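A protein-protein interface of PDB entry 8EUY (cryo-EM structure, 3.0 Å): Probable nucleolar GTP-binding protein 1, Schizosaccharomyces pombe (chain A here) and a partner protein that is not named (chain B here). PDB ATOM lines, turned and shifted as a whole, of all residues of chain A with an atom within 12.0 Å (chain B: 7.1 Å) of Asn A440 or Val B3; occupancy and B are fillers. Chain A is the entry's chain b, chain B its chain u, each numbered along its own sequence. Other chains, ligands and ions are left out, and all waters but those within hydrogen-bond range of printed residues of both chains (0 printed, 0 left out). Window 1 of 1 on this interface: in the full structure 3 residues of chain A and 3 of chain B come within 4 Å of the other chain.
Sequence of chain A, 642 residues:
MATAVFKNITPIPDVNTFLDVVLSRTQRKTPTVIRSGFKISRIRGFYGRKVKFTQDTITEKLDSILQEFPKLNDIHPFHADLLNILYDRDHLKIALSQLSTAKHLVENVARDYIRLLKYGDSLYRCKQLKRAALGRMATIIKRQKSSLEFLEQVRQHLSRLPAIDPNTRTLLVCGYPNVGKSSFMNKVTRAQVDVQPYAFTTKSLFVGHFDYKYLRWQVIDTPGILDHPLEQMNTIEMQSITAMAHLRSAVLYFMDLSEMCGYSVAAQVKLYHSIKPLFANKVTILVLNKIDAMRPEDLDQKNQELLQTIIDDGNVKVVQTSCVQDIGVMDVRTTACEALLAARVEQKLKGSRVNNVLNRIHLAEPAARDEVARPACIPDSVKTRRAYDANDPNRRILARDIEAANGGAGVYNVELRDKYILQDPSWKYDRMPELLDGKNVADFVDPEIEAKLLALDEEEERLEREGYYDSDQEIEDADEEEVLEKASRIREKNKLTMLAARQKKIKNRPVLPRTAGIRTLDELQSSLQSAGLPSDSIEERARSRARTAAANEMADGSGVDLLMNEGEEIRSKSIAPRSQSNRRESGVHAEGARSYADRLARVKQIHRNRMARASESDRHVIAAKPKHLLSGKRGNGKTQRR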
ATOM      1  N   MET A 432      -2.553 -18.744   7.888  1.00  0.00           N
ATOM      2  CA  MET A 432      -2.466 -19.049   6.472  1.00  0.00           C
ATOM      3  C   MET A 432      -3.766 -18.678   5.771  1.00  0.00           C
ATOM      4  O   MET A 432      -4.827 -18.632   6.402  1.00  0.00           O
ATOM      5  CB  MET A 432      -2.169 -20.537   6.240  1.00  0.00           C
ATOM      6  N   PRO A 433      -3.714 -18.394   4.469  1.00  0.00           N
ATOM      7  CA  PRO A 433      -4.942 -18.036   3.749  1.00  0.00           C
ATOM      8  C   PRO A 433      -5.943 -19.183   3.748  1.00  0.00           C
ATOM      9  O   PRO A 433      -5.576 -20.356   3.647  1.00  0.00           O
ATOM     10  CB  PRO A 433      -4.443 -17.721   2.334  1.00  0.00           C
ATOM     11  N   GLU A 434      -7.221 -18.829   3.862  1.00  0.00           N
ATOM     12  CA  GLU A 434      -8.312 -19.795   3.851  1.00  0.00           C
ATOM     13  C   GLU A 434      -9.118 -19.753   2.561  1.00  0.00           C
ATOM     14  O   GLU A 434      -9.279 -20.781   1.897  1.00  0.00           O
ATOM     15  CB  GLU A 434      -9.240 -19.554   5.050  1.00  0.00           C
ATOM     16  N   LEU A 435      -9.629 -18.583   2.188  1.00  0.00           N
ATOM     17  CA  LEU A 435     -10.391 -18.416   0.960  1.00  0.00           C
ATOM     18  C   LEU A 435      -9.901 -17.170   0.243  1.00  0.00           C
ATOM     19  O   LEU A 435      -9.645 -16.142   0.876  1.00  0.00           O
ATOM     20  CB  LEU A 435     -11.895 -18.310   1.241  1.00  0.00           C
ATOM     21  N   LEU A 436      -9.769 -17.267  -1.078  1.00  0.00           N
ATOM     22  CA  LEU A 436      -9.267 -16.156  -1.874  1.00  0.00           C
ATOM     23  C   LEU A 436      -9.977 -16.140  -3.218  1.00  0.00           C
ATOM     24  O   LEU A 436      -9.974 -17.149  -3.931  1.00  0.00           O
ATOM     25  CB  LEU A 436      -7.750 -16.265  -2.073  1.00  0.00           C
ATOM     26  N   ASP A 437     -10.569 -14.993  -3.558  1.00  0.00           N
ATOM     27  CA  ASP A 437     -11.273 -14.807  -4.828  1.00  0.00           C
ATOM     28  C   ASP A 437     -12.357 -15.864  -5.031  1.00  0.00           C
ATOM     29  O   ASP A 437     -12.511 -16.424  -6.118  1.00  0.00           O
ATOM     30  CB  ASP A 437     -10.296 -14.798  -6.006  1.00  0.00           C
ATOM     31  N   GLY A 438     -13.104 -16.156  -3.968  1.00  0.00           N
ATOM     32  CA  GLY A 438     -14.187 -17.112  -4.052  1.00  0.00           C
ATOM     33  C   GLY A 438     -13.762 -18.561  -4.061  1.00  0.00           C
ATOM     34  O   GLY A 438     -14.618 -19.440  -4.212  1.00  0.00           O
ATOM     35  N   LYS A 439     -12.471 -18.840  -3.904  1.00  0.00           N
ATOM     36  CA  LYS A 439     -11.944 -20.194  -3.917  1.00  0.00           C
ATOM     37  C   LYS A 439     -11.245 -20.480  -2.596  1.00  0.00           C
ATOM     38  O   LYS A 439     -10.504 -19.637  -2.081  1.00  0.00           O
ATOM     39  CB  LYS A 439     -10.970 -20.399  -5.083  1.00  0.00           C
ATOM     40  N   ASN A 440     -11.482 -21.671  -2.055  1.00  0.00           N
ATOM     41  CA  ASN A 440     -10.900 -22.069  -0.776  1.00  0.00           C
ATOM     42  C   ASN A 440      -9.407 -22.302  -0.964  1.00  0.00           C
ATOM     43  O   ASN A 440      -8.985 -23.341  -1.475  1.00  0.00           O
ATOM     44  CB  ASN A 440     -11.591 -23.319  -0.245  1.00  0.00           C
ATOM     45  N   VAL A 441      -8.599 -21.322  -0.552  1.00  0.00           N
ATOM     46  CA  VAL A 441      -7.149 -21.446  -0.678  1.00  0.00           C
ATOM     47  C   VAL A 441      -6.632 -22.579   0.199  1.00  0.00           C
ATOM     48  O   VAL A 441      -5.767 -23.361  -0.216  1.00  0.00           O
ATOM     49  CB  VAL A 441      -6.467 -20.110  -0.335  1.00  0.00           C
ATOM     50  N   ALA A 442      -7.149 -22.685   1.425  1.00  0.00           N
ATOM     51  CA  ALA A 442      -6.698 -23.734   2.334  1.00  0.00           C
ATOM     52  C   ALA A 442      -7.077 -25.121   1.832  1.00  0.00           C
ATOM     53  O   ALA A 442      -6.339 -26.085   2.065  1.00  0.00           O
ATOM     54  CB  ALA A 442      -7.271 -23.500   3.732  1.00  0.00           C
ATOM     55  N   ASP A 443      -8.213 -25.245   1.149  1.00  0.00           N
ATOM     56  CA  ASP A 443      -8.676 -26.529   0.639  1.00  0.00           C
ATOM     57  C   ASP A 443      -8.179 -26.824  -0.770  1.00  0.00           C
ATOM     58  O   ASP A 443      -8.539 -27.864  -1.332  1.00  0.00           O
ATOM     59  CB  ASP A 443     -10.206 -26.586   0.666  1.00  0.00           C
ATOM     60  N   PHE A 444      -7.366 -25.940  -1.357  1.00  0.00           N
ATOM     61  CA  PHE A 444      -6.835 -26.148  -2.698  1.00  0.00           C
ATOM     62  C   PHE A 444      -5.319 -25.991  -2.743  1.00  0.00           C
ATOM     63  O   PHE A 444      -4.754 -25.785  -3.822  1.00  0.00           O
ATOM     64  CB  PHE A 444      -7.493 -25.191  -3.697  1.00  0.00           C
ATOM     65  N   VAL A 445      -4.649 -26.085  -1.599  1.00  0.00           N
ATOM     66  CA  VAL A 445      -3.200 -25.955  -1.548  1.00  0.00           C
ATOM     67  C   VAL A 445      -2.571 -27.245  -1.036  1.00  0.00           C
ATOM     68  O   VAL A 445      -2.991 -27.787  -0.013  1.00  0.00           O
ATOM     69  CB  VAL A 445      -2.777 -24.761  -0.675  1.00  0.00           C
ATOM     70  N   MET B   1     -11.762 -21.484   6.270  1.00  0.00           N
ATOM     71  CA  MET B   1     -12.997 -21.247   5.532  1.00  0.00           C
ATOM     72  C   MET B   1     -12.943 -21.892   4.152  1.00  0.00           C
ATOM     73  O   MET B   1     -11.956 -21.752   3.428  1.00  0.00           O
ATOM     74  CB  MET B   1     -13.264 -19.745   5.403  1.00  0.00           C
ATOM     75  N   ARG B   2     -14.011 -22.599   3.793  1.00  0.00           N
ATOM     76  CA  ARG B   2     -14.117 -23.277   2.507  1.00  0.00           C
ATOM     77  C   ARG B   2     -15.376 -22.807   1.796  1.00  0.00           C
ATOM     78  O   ARG B   2     -16.456 -22.775   2.395  1.00  0.00           O
ATOM     79  CB  ARG B   2     -14.143 -24.798   2.687  1.00  0.00           C
ATOM     80  N   VAL B   3     -15.235 -22.446   0.525  1.00  0.00           N
ATOM     81  CA  VAL B   3     -16.355 -21.974  -0.282  1.00  0.00           C
ATOM     82  C   VAL B   3     -16.984 -23.185  -0.963  1.00  0.00           C
ATOM     83  O   VAL B   3     -16.409 -23.756  -1.893  1.00  0.00           O
ATOM     84  CB  VAL B   3     -15.907 -20.928  -1.309  1.00  0.00           C
ATOM     85  N   HIS B   4     -18.166 -23.576  -0.498  1.00  0.00           N
ATOM     86  CA  HIS B   4     -18.859 -24.724  -1.059  1.00  0.00           C
ATOM     87  C   HIS B   4     -19.472 -24.375  -2.412  1.00  0.00           C
ATOM     88  O   HIS B   4     -19.606 -23.207  -2.785  1.00  0.00           O
ATOM     89  CB  HIS B   4     -19.945 -25.217  -0.102  1.00  0.00           C
ATOM     90  N   THR B   5     -19.846 -25.416  -3.150  1.00  0.00           N
ATOM     91  CA  THR B   5     -20.457 -25.277  -4.464  1.00  0.00           C
ATOM     92  C   THR B   5     -21.941 -25.604  -4.378  1.00  0.00           C
ATOM     93  O   THR B   5     -22.337 -26.573  -3.722  1.00  0.00           O
ATOM     94  CB  THR B   5     -19.782 -26.194  -5.488  1.00  0.00           C
ATOM     95  N   GLY B  11     -22.866 -22.856  -8.064  1.00  0.00           N
ATOM     96  CA  GLY B  11     -22.143 -21.645  -7.767  1.00  0.00           C
ATOM     97  C   GLY B  11     -21.517 -21.652  -6.389  1.00  0.00           C
ATOM     98  O   GLY B  11     -21.830 -22.494  -5.540  1.00  0.00           O
ATOM     99  N   PRO B  12     -20.609 -20.708  -6.143  1.00  0.00           N
ATOM    100  CA  PRO B  12     -19.965 -20.633  -4.828  1.00  0.00           C
ATOM    101  C   PRO B  12     -20.969 -20.303  -3.736  1.00  0.00           C
ATOM    102  O   PRO B  12     -21.932 -19.562  -3.946  1.00  0.00           O
ATOM    103  CB  PRO B  12     -18.935 -19.511  -5.001  1.00  0.00           C
ATOM    104  N   VAL B  13     -20.729 -20.863  -2.554  1.00  0.00           N
ATOM    105  CA  VAL B  13     -21.575 -20.648  -1.387  1.00  0.00           C
ATOM    106  C   VAL B  13     -20.742 -19.954  -0.321  1.00  0.00           C
ATOM    107  O   VAL B  13     -19.682 -20.456   0.071  1.00  0.00           O
ATOM    108  CB  VAL B  13     -22.156 -21.970  -0.853  1.00  0.00           C
ATOM    109  N   TYR B  14     -21.218 -18.808   0.143  1.00  0.00           N
ATOM    110  CA  TYR B  14     -20.549 -18.030   1.168  1.00  0.00           C
ATOM    111  C   TYR B  14     -21.275 -18.163   2.498  1.00  0.00           C
ATOM    112  O   TYR B  14     -22.472 -18.468   2.539  1.00  0.00           O
ATOM    113  CB  TYR B  14     -20.477 -16.549   0.769  1.00  0.00           C
ATOM    114  N   PRO B  15     -20.575 -17.958   3.613  1.00  0.00           N
ATOM    115  CA  PRO B  15     -21.237 -18.052   4.919  1.00  0.00           C
ATOM    116  C   PRO B  15     -22.343 -17.015   5.054  1.00  0.00           C
ATOM    117  O   PRO B  15     -22.232 -15.891   4.561  1.00  0.00           O
ATOM    118  CB  PRO B  15     -20.098 -17.798   5.912  1.00  0.00           C
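The backbone NH of Val A441 lies within hydrogen-bond range of the backbone carbonyl oxygen of Glu A434. O of Glu A434 sits at hydrogen-bond distance from N of Ala A442, 2.9 Å away.
Of the 10 printed residues of chain B, 3 touch a printed residue of chain A. Printed residues of chain B that touch a printed residue of chain A: Met B1, Arg B2 and Val B3. Of the 14 printed residues of chain A, 3 touch a printed residue of chain B. Among the printed residues, 4 pairs touch across the chains.
Gly A438 touches Val B3. Asn A440 touches Arg B2. Val B3 touches Asn A440.
O of Glu A434 lies close to O of Met B1 (3.2 Å).
Printed residues of chain B within 4 Å of Asn A440: Arg B2 (3.7 Å) and Val B3 (3.8 Å). Of chain A, only Gly A438 (3.5 Å) and Asn A440 (3.8 Å) come within 4 Å of Val B3. Arg B2 touches one residue of chain A. No residue of chain A comes within 4 Å of His B4. No residue of chain A comes within 4 Å of Thr B5. Pro B12 touches none of the printed residues of chain A. No residue of chain A comes within 4 Å of Val B13. Of the printed residues of chain B, Gly A438 touches Val B3 (3.5 Å). Printed residues of chain B within 4 Å of Glu A434: Met B1 (3.2 Å). Printed residues of chain A within 4 Å of Met B1: Glu A434. Asp A443 touches none of the printed residues of chain B. Leu A436 touches none of the printed residues of chain B. The nearest printed residue of chain B that does not touch Asn A440 is Met B1 (4.01 Å).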
